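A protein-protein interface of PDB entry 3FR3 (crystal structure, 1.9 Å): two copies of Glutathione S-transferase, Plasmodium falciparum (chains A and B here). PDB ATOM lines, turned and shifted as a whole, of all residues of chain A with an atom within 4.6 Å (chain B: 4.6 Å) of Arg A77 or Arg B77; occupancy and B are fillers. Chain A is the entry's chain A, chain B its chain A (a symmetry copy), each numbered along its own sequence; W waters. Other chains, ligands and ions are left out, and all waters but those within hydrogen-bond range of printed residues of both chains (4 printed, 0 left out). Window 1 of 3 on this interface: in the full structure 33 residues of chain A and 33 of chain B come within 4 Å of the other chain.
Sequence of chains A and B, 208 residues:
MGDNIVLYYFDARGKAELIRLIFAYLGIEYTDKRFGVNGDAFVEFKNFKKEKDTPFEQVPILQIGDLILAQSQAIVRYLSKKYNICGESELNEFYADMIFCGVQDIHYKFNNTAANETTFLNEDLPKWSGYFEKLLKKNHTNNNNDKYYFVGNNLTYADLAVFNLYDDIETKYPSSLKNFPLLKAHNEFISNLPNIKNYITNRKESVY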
ATOM      1  N   GLN A  73      24.610  10.961  -6.395  1.00  0.00           N
ATOM      2  CA  GLN A  73      25.321  12.278  -6.491  1.00  0.00           C
ATOM      3  C   GLN A  73      24.708  13.165  -7.519  1.00  0.00           C
ATOM      4  O   GLN A  73      24.672  14.363  -7.356  1.00  0.00           O
ATOM      5  CB  GLN A  73      26.759  12.073  -6.965  1.00  0.00           C
ATOM      6  CG  GLN A  73      27.583  11.424  -5.952  1.00  0.00           C
ATOM      7  CD  GLN A  73      29.082  11.403  -6.376  1.00  0.00           C
ATOM      8  OE1 GLN A  73      29.766  10.469  -5.999  1.00  0.00           O
ATOM      9  NE2 GLN A  73      29.570  12.416  -7.166  1.00  0.00           N
ATOM     10  N   ALA A  74      24.298  12.585  -8.646  1.00  0.00           N
ATOM     11  CA  ALA A  74      23.656  13.356  -9.692  1.00  0.00           C
ATOM     12  C   ALA A  74      22.300  13.903  -9.236  1.00  0.00           C
ATOM     13  O   ALA A  74      21.933  15.027  -9.620  1.00  0.00           O
ATOM     14  CB  ALA A  74      23.485  12.426 -10.987  1.00  0.00           C
ATOM     15  N   ILE A  75      21.550  13.121  -8.450  1.00  0.00           N
ATOM     16  CA  ILE A  75      20.259  13.604  -7.880  1.00  0.00           C
ATOM     17  C   ILE A  75      20.547  14.771  -6.958  1.00  0.00           C
ATOM     18  O   ILE A  75      19.885  15.805  -7.003  1.00  0.00           O
ATOM     19  CB  ILE A  75      19.515  12.434  -7.120  1.00  0.00           C
ATOM     20  CG1 ILE A  75      19.025  11.364  -8.138  1.00  0.00           C
ATOM     21  CG2 ILE A  75      18.327  12.936  -6.291  1.00  0.00           C
ATOM     22  CD1 ILE A  75      18.784   9.997  -7.536  1.00  0.00           C
ATOM     23  N   VAL A  76      21.540  14.599  -6.090  1.00  0.00           N
ATOM     24  CA  VAL A  76      21.921  15.693  -5.151  1.00  0.00           C
ATOM     25  C   VAL A  76      22.194  16.950  -5.932  1.00  0.00           C
ATOM     26  O   VAL A  76      21.743  18.026  -5.522  1.00  0.00           O
ATOM     27  CB  VAL A  76      23.146  15.317  -4.264  1.00  0.00           C
ATOM     28  CG1 VAL A  76      23.788  16.548  -3.611  1.00  0.00           C
ATOM     29  CG2 VAL A  76      22.737  14.217  -3.193  1.00  0.00           C
ATOM     30  N   ARG A  77      23.016  16.842  -6.989  1.00  0.00           N
ATOM     31  CA  ARG A  77      23.446  18.033  -7.682  1.00  0.00           C
ATOM     32  C   ARG A  77      22.277  18.707  -8.376  1.00  0.00           C
ATOM     33  O   ARG A  77      22.177  19.924  -8.406  1.00  0.00           O
ATOM     34  CB  ARG A  77      24.577  17.710  -8.685  1.00  0.00           C
ATOM     35  CG  ARG A  77      25.986  17.748  -8.004  1.00  0.00           C
ATOM     36  CD  ARG A  77      27.112  17.460  -9.052  1.00  0.00           C
ATOM     37  NE  ARG A  77      27.100  16.039  -9.546  1.00  0.00           N
ATOM     38  CZ  ARG A  77      27.701  15.013  -8.931  1.00  0.00           C
ATOM     39  NH1 ARG A  77      28.345  15.185  -7.762  1.00  0.00           N
ATOM     40  NH2 ARG A  77      27.669  13.810  -9.490  1.00  0.00           N
ATOM     41  N   TYR A  78      21.400  17.892  -8.942  1.00  0.00           N
ATOM     42  CA  TYR A  78      20.222  18.396  -9.665  1.00  0.00           C
ATOM     43  C   TYR A  78      19.287  19.146  -8.727  1.00  0.00           C
ATOM     44  O   TYR A  78      18.811  20.261  -9.010  1.00  0.00           O
ATOM     45  CB  TYR A  78      19.500  17.140 -10.242  1.00  0.00           C
ATOM     46  CG  TYR A  78      18.129  17.438 -10.820  1.00  0.00           C
ATOM     47  CD1 TYR A  78      16.953  17.087 -10.120  1.00  0.00           C
ATOM     48  CD2 TYR A  78      18.003  18.049 -12.069  1.00  0.00           C
ATOM     49  CE1 TYR A  78      15.679  17.376 -10.671  1.00  0.00           C
ATOM     50  CE2 TYR A  78      16.736  18.327 -12.619  1.00  0.00           C
ATOM     51  CZ  TYR A  78      15.596  17.993 -11.903  1.00  0.00           C
ATOM     52  OH  TYR A  78      14.342  18.258 -12.447  1.00  0.00           O
ATOM     53  N   LEU A  79      18.981  18.517  -7.597  1.00  0.00           N
ATOM     54  CA  LEU A  79      18.136  19.128  -6.616  1.00  0.00           C
ATOM     55  C   LEU A  79      18.793  20.414  -6.078  1.00  0.00           C
ATOM     56  O   LEU A  79      18.103  21.398  -5.846  1.00  0.00           O
ATOM     57  CB  LEU A  79      17.972  18.157  -5.460  1.00  0.00           C
ATOM     58  CG  LEU A  79      16.850  17.125  -5.250  1.00  0.00           C
ATOM     59  CD1 LEU A  79      15.718  17.026  -6.253  1.00  0.00           C
ATOM     60  CD2 LEU A  79      17.045  15.891  -4.407  1.00  0.00           C
ATOM     61  N   SER A  80      20.119  20.387  -5.862  1.00  0.00           N
ATOM     62  CA  SER A  80      20.824  21.530  -5.232  1.00  0.00           C
ATOM     63  C   SER A  80      20.805  22.740  -6.175  1.00  0.00           C
ATOM     64  O   SER A  80      20.659  23.904  -5.761  1.00  0.00           O
ATOM     65  CB  SER A  80      22.237  21.140  -4.837  1.00  0.00           C
ATOM     66  OG  SER A  80      22.175  20.148  -3.812  1.00  0.00           O
ATOM     67  N   LYS A  81      20.891  22.443  -7.467  1.00  0.00           N
ATOM     68  CA  LYS A  81      20.819  23.485  -8.488  1.00  0.00           C
ATOM     69  C   LYS A  81      19.400  24.048  -8.576  1.00  0.00           C
ATOM     70  O   LYS A  81      19.239  25.263  -8.607  1.00  0.00           O
ATOM     71  CB  LYS A  81      21.270  22.943  -9.857  1.00  0.00           C
ATOM     72  CG  LYS A  81      21.181  23.904 -11.034  1.00  0.00           C
ATOM     73  CD  LYS A  81      22.498  23.834 -11.823  1.00  0.00           C
ATOM     74  CE  LYS A  81      22.409  24.551 -13.163  1.00  0.00           C
ATOM     75  NZ  LYS A  81      23.546  24.118 -14.072  1.00  0.00           N
ATOM     76  N   ASP A  97      31.087  21.403  -4.963  1.00  0.00           N
ATOM     77  CA  ASP A  97      31.237  20.096  -5.634  1.00  0.00           C
ATOM     78  C   ASP A  97      32.541  19.462  -5.138  1.00  0.00           C
ATOM     79  O   ASP A  97      32.573  18.271  -4.768  1.00  0.00           O
ATOM     80  CB  ASP A  97      31.383  20.396  -7.126  1.00  0.00           C
ATOM     81  CG  ASP A  97      31.218  19.177  -8.008  1.00  0.00           C
ATOM     82  OD1 ASP A  97      31.105  19.383  -9.240  1.00  0.00           O
ATOM     83  OD2 ASP A  97      31.297  18.035  -7.501  1.00  0.00           O
ATOM     84  N   PHE A 100      31.993  18.177  -1.629  1.00  0.00           N
ATOM     85  CA  PHE A 100      31.185  16.930  -1.676  1.00  0.00           C
ATOM     86  C   PHE A 100      32.009  15.740  -2.149  1.00  0.00           C
ATOM     87  O   PHE A 100      31.920  14.647  -1.596  1.00  0.00           O
ATOM     88  CB  PHE A 100      29.944  17.165  -2.562  1.00  0.00           C
ATOM     89  CG  PHE A 100      29.026  16.010  -2.636  1.00  0.00           C
ATOM     90  CD1 PHE A 100      28.665  15.318  -1.489  1.00  0.00           C
ATOM     91  CD2 PHE A 100      28.477  15.628  -3.854  1.00  0.00           C
ATOM     92  CE1 PHE A 100      27.794  14.228  -1.556  1.00  0.00           C
ATOM     93  CE2 PHE A 100      27.582  14.540  -3.934  1.00  0.00           C
ATOM     94  CZ  PHE A 100      27.249  13.846  -2.800  1.00  0.00           C
ATOM     95  N   CYS A 101      32.848  15.935  -3.179  1.00  0.00           N
ATOM     96  CA  CYS A 101      33.664  14.852  -3.665  1.00  0.00           C
ATOM     97  C   CYS A 101      34.653  14.369  -2.587  1.00  0.00           C
ATOM     98  O   CYS A 101      34.928  13.161  -2.475  1.00  0.00           O
ATOM     99  CB  CYS A 101      34.433  15.301  -4.928  1.00  0.00           C
ATOM    100  SG  CYS A 101      33.324  15.486  -6.364  1.00  0.00           S
ATOM    101  N   TYR A 157      24.639  22.190  -0.394  1.00  0.00           N
ATOM    102  CA  TYR A 157      24.555  20.751  -0.134  1.00  0.00           C
ATOM    103  C   TYR A 157      25.875  20.250   0.474  1.00  0.00           C
ATOM    104  O   TYR A 157      25.914  19.167   1.030  1.00  0.00           O
ATOM    105  CB  TYR A 157      24.239  19.954  -1.403  1.00  0.00           C
ATOM    106  CG  TYR A 157      25.276  20.032  -2.522  1.00  0.00           C
ATOM    107  CD1 TYR A 157      26.110  18.921  -2.800  1.00  0.00           C
ATOM    108  CD2 TYR A 157      25.355  21.197  -3.359  1.00  0.00           C
ATOM    109  CE1 TYR A 157      27.044  18.960  -3.820  1.00  0.00           C
ATOM    110  CE2 TYR A 157      26.325  21.231  -4.447  1.00  0.00           C
ATOM    111  CZ  TYR A 157      27.121  20.075  -4.634  1.00  0.00           C
ATOM    112  OH  TYR A 157      28.054  20.006  -5.609  1.00  0.00           O
ATOM    113  N   GLN B  73      36.352  14.655 -10.462  1.00  0.00           N
ATOM    114  CA  GLN B  73      34.961  14.797 -11.005  1.00  0.00           C
ATOM    115  C   GLN B  73      34.499  16.213 -10.985  1.00  0.00           C
ATOM    116  O   GLN B  73      33.779  16.638 -11.859  1.00  0.00           O
ATOM    117  CB  GLN B  73      33.965  14.053 -10.116  1.00  0.00           C
ATOM    118  CG  GLN B  73      34.118  12.606 -10.211  1.00  0.00           C
ATOM    119  CD  GLN B  73      32.973  11.870  -9.455  1.00  0.00           C
ATOM    120  OE1 GLN B  73      33.227  10.790  -8.950  1.00  0.00           O
ATOM    121  NE2 GLN B  73      31.736  12.462  -9.368  1.00  0.00           N
ATOM    122  N   ALA B  74      34.841  16.942  -9.923  1.00  0.00           N
ATOM    123  CA  ALA B  74      34.471  18.340  -9.827  1.00  0.00           C
ATOM    124  C   ALA B  74      35.178  19.183 -10.892  1.00  0.00           C
ATOM    125  O   ALA B  74      34.577  20.136 -11.417  1.00  0.00           O
ATOM    126  CB  ALA B  74      34.829  18.868  -8.356  1.00  0.00           C
ATOM    127  N   ILE B  75      36.442  18.864 -11.195  1.00  0.00           N
ATOM    128  CA  ILE B  75      37.180  19.567 -12.284  1.00  0.00           C
ATOM    129  C   ILE B  75      36.476  19.292 -13.597  1.00  0.00           C
ATOM    130  O   ILE B  75      36.236  20.191 -14.399  1.00  0.00           O
ATOM    131  CB  ILE B  75      38.689  19.096 -12.326  1.00  0.00           C
ATOM    132  CG1 ILE B  75      39.442  19.604 -11.063  1.00  0.00           C
ATOM    133  CG2 ILE B  75      39.419  19.578 -13.586  1.00  0.00           C
ATOM    134  CD1 ILE B  75      40.687  18.817 -10.721  1.00  0.00           C
ATOM    135  N   VAL B  76      36.155  18.024 -13.834  1.00  0.00           N
ATOM    136  CA  VAL B  76      35.440  17.646 -15.087  1.00  0.00           C
ATOM    137  C   VAL B  76      34.192  18.478 -15.221  1.00  0.00           C
ATOM    138  O   VAL B  76      33.911  18.973 -16.318  1.00  0.00           O
ATOM    139  CB  VAL B  76      35.099  16.127 -15.145  1.00  0.00           C
ATOM    140  CG1 VAL B  76      34.029  15.812 -16.199  1.00  0.00           C
ATOM    141  CG2 VAL B  76      36.420  15.271 -15.359  1.00  0.00           C
ATOM    142  N   ARG B  77      33.390  18.546 -14.147  1.00  0.00           N
ATOM    143  CA  ARG B  77      32.103  19.191 -14.258  1.00  0.00           C
ATOM    144  C   ARG B  77      32.264  20.679 -14.510  1.00  0.00           C
ATOM    145  O   ARG B  77      31.519  21.274 -15.273  1.00  0.00           O
ATOM    146  CB  ARG B  77      31.244  18.930 -12.999  1.00  0.00           C
ATOM    147  CG  ARG B  77      30.442  17.591 -13.110  1.00  0.00           C
ATOM    148  CD  ARG B  77      29.551  17.375 -11.841  1.00  0.00           C
ATOM    149  NE  ARG B  77      30.356  17.095 -10.602  1.00  0.00           N
ATOM    150  CZ  ARG B  77      30.798  15.885 -10.238  1.00  0.00           C
ATOM    151  NH1 ARG B  77      30.578  14.804 -11.010  1.00  0.00           N
ATOM    152  NH2 ARG B  77      31.454  15.748  -9.093  1.00  0.00           N
ATOM    153  N   TYR B  78      33.246  21.270 -13.845  1.00  0.00           N
ATOM    154  CA  TYR B  78      33.517  22.710 -13.974  1.00  0.00           C
ATOM    155  C   TYR B  78      33.939  23.060 -15.394  1.00  0.00           C
ATOM    156  O   TYR B  78      33.449  24.018 -16.019  1.00  0.00           O
ATOM    157  CB  TYR B  78      34.680  23.019 -12.983  1.00  0.00           C
ATOM    158  CG  TYR B  78      35.263  24.410 -13.144  1.00  0.00           C
ATOM    159  CD1 TYR B  78      36.512  24.607 -13.776  1.00  0.00           C
ATOM    160  CD2 TYR B  78      34.584  25.526 -12.652  1.00  0.00           C
ATOM    161  CE1 TYR B  78      37.042  25.914 -13.924  1.00  0.00           C
ATOM    162  CE2 TYR B  78      35.117  26.823 -12.791  1.00  0.00           C
ATOM    163  CZ  TYR B  78      36.334  26.993 -13.435  1.00  0.00           C
ATOM    164  OH  TYR B  78      36.867  28.271 -13.567  1.00  0.00           O
ATOM    165  N   LEU B  79      34.895  22.296 -15.914  1.00  0.00           N
ATOM    166  CA  LEU B  79      35.358  22.502 -17.252  1.00  0.00           C
ATOM    167  C   LEU B  79      34.209  22.272 -18.253  1.00  0.00           C
ATOM    168  O   LEU B  79      34.102  22.997 -19.233  1.00  0.00           O
ATOM    169  CB  LEU B  79      36.449  21.485 -17.538  1.00  0.00           C
ATOM    170  CG  LEU B  79      37.969  21.665 -17.374  1.00  0.00           C
ATOM    171  CD1 LEU B  79      38.527  22.995 -16.911  1.00  0.00           C
ATOM    172  CD2 LEU B  79      38.896  20.494 -17.165  1.00  0.00           C
ATOM    173  N   SER B  80      33.373  21.248 -18.009  1.00  0.00           N
ATOM    174  CA  SER B  80      32.311  20.870 -18.974  1.00  0.00           C
ATOM    175  C   SER B  80      31.250  21.976 -19.045  1.00  0.00           C
ATOM    176  O   SER B  80      30.701  22.303 -20.112  1.00  0.00           O
ATOM    177  CB  SER B  80      31.707  19.526 -18.610  1.00  0.00           C
ATOM    178  OG  SER B  80      32.704  18.514 -18.757  1.00  0.00           O
ATOM    179  N   LYS B  81      31.014  22.597 -17.895  1.00  0.00           N
ATOM    180  CA  LYS B  81      30.077  23.716 -17.820  1.00  0.00           C
ATOM    181  C   LYS B  81      30.660  24.946 -18.517  1.00  0.00           C
ATOM    182  O   LYS B  81      29.959  25.581 -19.296  1.00  0.00           O
ATOM    183  CB  LYS B  81      29.728  24.041 -16.356  1.00  0.00           C
ATOM    184  CG  LYS B  81      28.812  25.235 -16.123  1.00  0.00           C
ATOM    185  CD  LYS B  81      27.720  24.824 -15.123  1.00  0.00           C
ATOM    186  CE  LYS B  81      26.918  26.017 -14.618  1.00  0.00           C
ATOM    187  NZ  LYS B  81      26.155  25.646 -13.358  1.00  0.00           N
ATOM    188  N   ASP B  97      25.378  13.857 -16.117  1.00  0.00           N
ATOM    189  CA  ASP B  97      25.945  13.627 -14.772  1.00  0.00           C
ATOM    190  C   ASP B  97      25.607  12.189 -14.361  1.00  0.00           C
ATOM    191  O   ASP B  97      26.480  11.439 -13.881  1.00  0.00           O
ATOM    192  CB  ASP B  97      25.213  14.583 -13.830  1.00  0.00           C
ATOM    193  CG  ASP B  97      25.878  14.730 -12.479  1.00  0.00           C
ATOM    194  OD1 ASP B  97      25.463  15.656 -11.743  1.00  0.00           O
ATOM    195  OD2 ASP B  97      26.726  13.883 -12.116  1.00  0.00           O
ATOM    196  N   PHE B 100      27.852   9.833 -16.276  1.00  0.00           N
ATOM    197  CA  PHE B 100      29.224   9.874 -15.701  1.00  0.00           C
ATOM    198  C   PHE B 100      29.304   9.123 -14.378  1.00  0.00           C
ATOM    199  O   PHE B 100      30.248   8.381 -14.128  1.00  0.00           O
ATOM    200  CB  PHE B 100      29.668  11.345 -15.562  1.00  0.00           C
ATOM    201  CG  PHE B 100      31.047  11.513 -15.056  1.00  0.00           C
ATOM    202  CD1 PHE B 100      32.086  10.750 -15.566  1.00  0.00           C
ATOM    203  CD2 PHE B 100      31.326  12.474 -14.091  1.00  0.00           C
ATOM    204  CE1 PHE B 100      33.390  10.911 -15.092  1.00  0.00           C
ATOM    205  CE2 PHE B 100      32.642  12.660 -13.616  1.00  0.00           C
ATOM    206  CZ  PHE B 100      33.659  11.884 -14.107  1.00  0.00           C
ATOM    207  N   CYS B 101      28.296   9.290 -13.507  1.00  0.00           N
ATOM    208  CA  CYS B 101      28.308   8.599 -12.244  1.00  0.00           C
ATOM    209  C   CYS B 101      28.256   7.071 -12.441  1.00  0.00           C
ATOM    210  O   CYS B 101      28.898   6.313 -11.693  1.00  0.00           O
ATOM    211  CB  CYS B 101      27.113   9.063 -11.381  1.00  0.00           C
ATOM    212  SG  CYS B 101      27.341  10.767 -10.772  1.00  0.00           S
ATOM    213  N   TYR B 157      30.639  15.616 -21.800  1.00  0.00           N
ATOM    214  CA  TYR B 157      31.725  14.906 -21.119  1.00  0.00           C
ATOM    215  C   TYR B 157      31.320  13.445 -20.868  1.00  0.00           C
ATOM    216  O   TYR B 157      32.171  12.619 -20.588  1.00  0.00           O
ATOM    217  CB  TYR B 157      32.103  15.570 -19.792  1.00  0.00           C
ATOM    218  CG  TYR B 157      31.010  15.612 -18.725  1.00  0.00           C
ATOM    219  CD1 TYR B 157      31.088  14.767 -17.591  1.00  0.00           C
ATOM    220  CD2 TYR B 157      29.941  16.568 -18.817  1.00  0.00           C
ATOM    221  CE1 TYR B 157      30.121  14.798 -16.602  1.00  0.00           C
ATOM    222  CE2 TYR B 157      28.933  16.616 -17.765  1.00  0.00           C
ATOM    223  CZ  TYR B 157      29.095  15.721 -16.680  1.00  0.00           C
ATOM    224  OH  TYR B 157      28.213  15.680 -15.657  1.00  0.00           O
HETATM  225  O   HOH W   1      32.505  21.522 -10.347  1.00  0.00           O
HETATM  226  O   HOH W   2      22.758  16.314 -11.860  1.00  0.00           O
HETATM  227  O   HOH W   3      29.211   9.117  -8.264  1.00  0.00           O
HETATM  228  O   HOH W   4      33.850  11.999  -6.623  1.00  0.00           O
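Gln B73 touches its own counterpart, Gln A73. Arg B77 touches its own counterpart, Arg A77. Arg A77 touches Cys B101, and with the chains exchanged Cys A101 touches Arg B77. Lys A81 touches its own counterpart, Lys B81. Of the 9 pairs that touch across the chains among the printed residues, 9 have their exchanged pair printed and touching as well.
NH1 of Arg B77 sits close to NE2 of Gln B73 (3.1 Å). OH of Tyr A157 sits close to N of Asp A97 (3.4 Å). The backbone NH of Asp B97 lies close to the side-chain hydroxyl of Tyr B157 (3.4 Å). The backbone carbonyl oxygen (O) of Asp B97 sits at hydrogen-bond distance from the side-chain sulfur (SG) of Cys B101, 3.3 Å away. The backbone carbonyl oxygen of Asp A97 is in hydrogen-bond range of the side-chain sulfur of Cys A101. The side-chain amide nitrogen (NE2) of Gln A73 lies close to the guanidinium group (NH1) of Arg A77 (3.1 Å).
The side-chain carboxylate (OD1) of Asp A97 is in salt-bridge range of the guanidinium group (NE) of Arg B77 (2.8 Å). NE of Arg A77 lies within salt-bridge range of OD1 of Asp B97, 2.8 Å away. The guanidinium group (NH2) of Arg A77 is in hydrogen-bond range of the side-chain sulfur (SG) of Cys B101 (3.3 Å). The side-chain amino group (NZ) of Lys B81 sits close to the side-chain amino group (NZ) of Lys A81, at 3.1 Å. The guanidinium group (NH1) of Arg A77 lies close to the guanidinium group (NH2) of Arg B77 (3.4 Å). The side-chain amide nitrogen of Gln A73 sits close to the side-chain amide nitrogen of Gln B73 (3.1 Å). NH2 of Arg B77 lies within hydrogen-bond range of SG of Cys A101, at 3.3 Å.
Of chain B, only Arg B77 (3.4 Å), Asp B97 (2.8 Å) and Cys B101 (3.3 Å) come within 4 Å of Arg A77. Printed residues of chain B within 4 Å of Cys A101: Arg B77. Printed residues of chain A within 4 Å of Gln B73: Gln A73 (3.1 Å). Of the printed residues of chain A, Ala B74 touches Asp A97. Arg B77 touches just these residues of chain A: Arg A77, Asp A97 and Cys A101. Of the printed residues of chain A, Lys B81 touches Lys A81 (3.1 Å).
CA of Ala A74 touches OD1 of Asp B97, 3.6 Å away. CA of Ala B74 touches OD1 of Asp A97 (3.6 Å).
Water W3 bridges OE1 of Gln A73 and SG of Cys B101. Water W4 bridges the side-chain amide oxygen of Gln B73 (2.7 Å) and the side-chain sulfur of Cys A101 (3.5 Å). Water W1 lies within hydrogen-bond range of O of Ala B74 and OD1 of Asp A97. Water W2 lies within hydrogen-bond range of O of Ala A74 (2.7 Å) and OD1 of Asp B97 (2.8 Å).
Of the 13 printed residues of chain A, 6 touch a printed residue of chain B. Printed residues of chain A that touch a printed residue of chain B: Gln A73, Ala A74, Arg A77, Lys A81, Asp A97 and Cys A101. Hydrophobic or aromatic side chains of chain A within 4 Å of the printed part of chain B: Ala A74. Along chain A the printed residues that touch a printed residue of chain B span positions 73 to 101. Of the 13 printed residues of chain B, 6 touch a printed residue of chain A.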
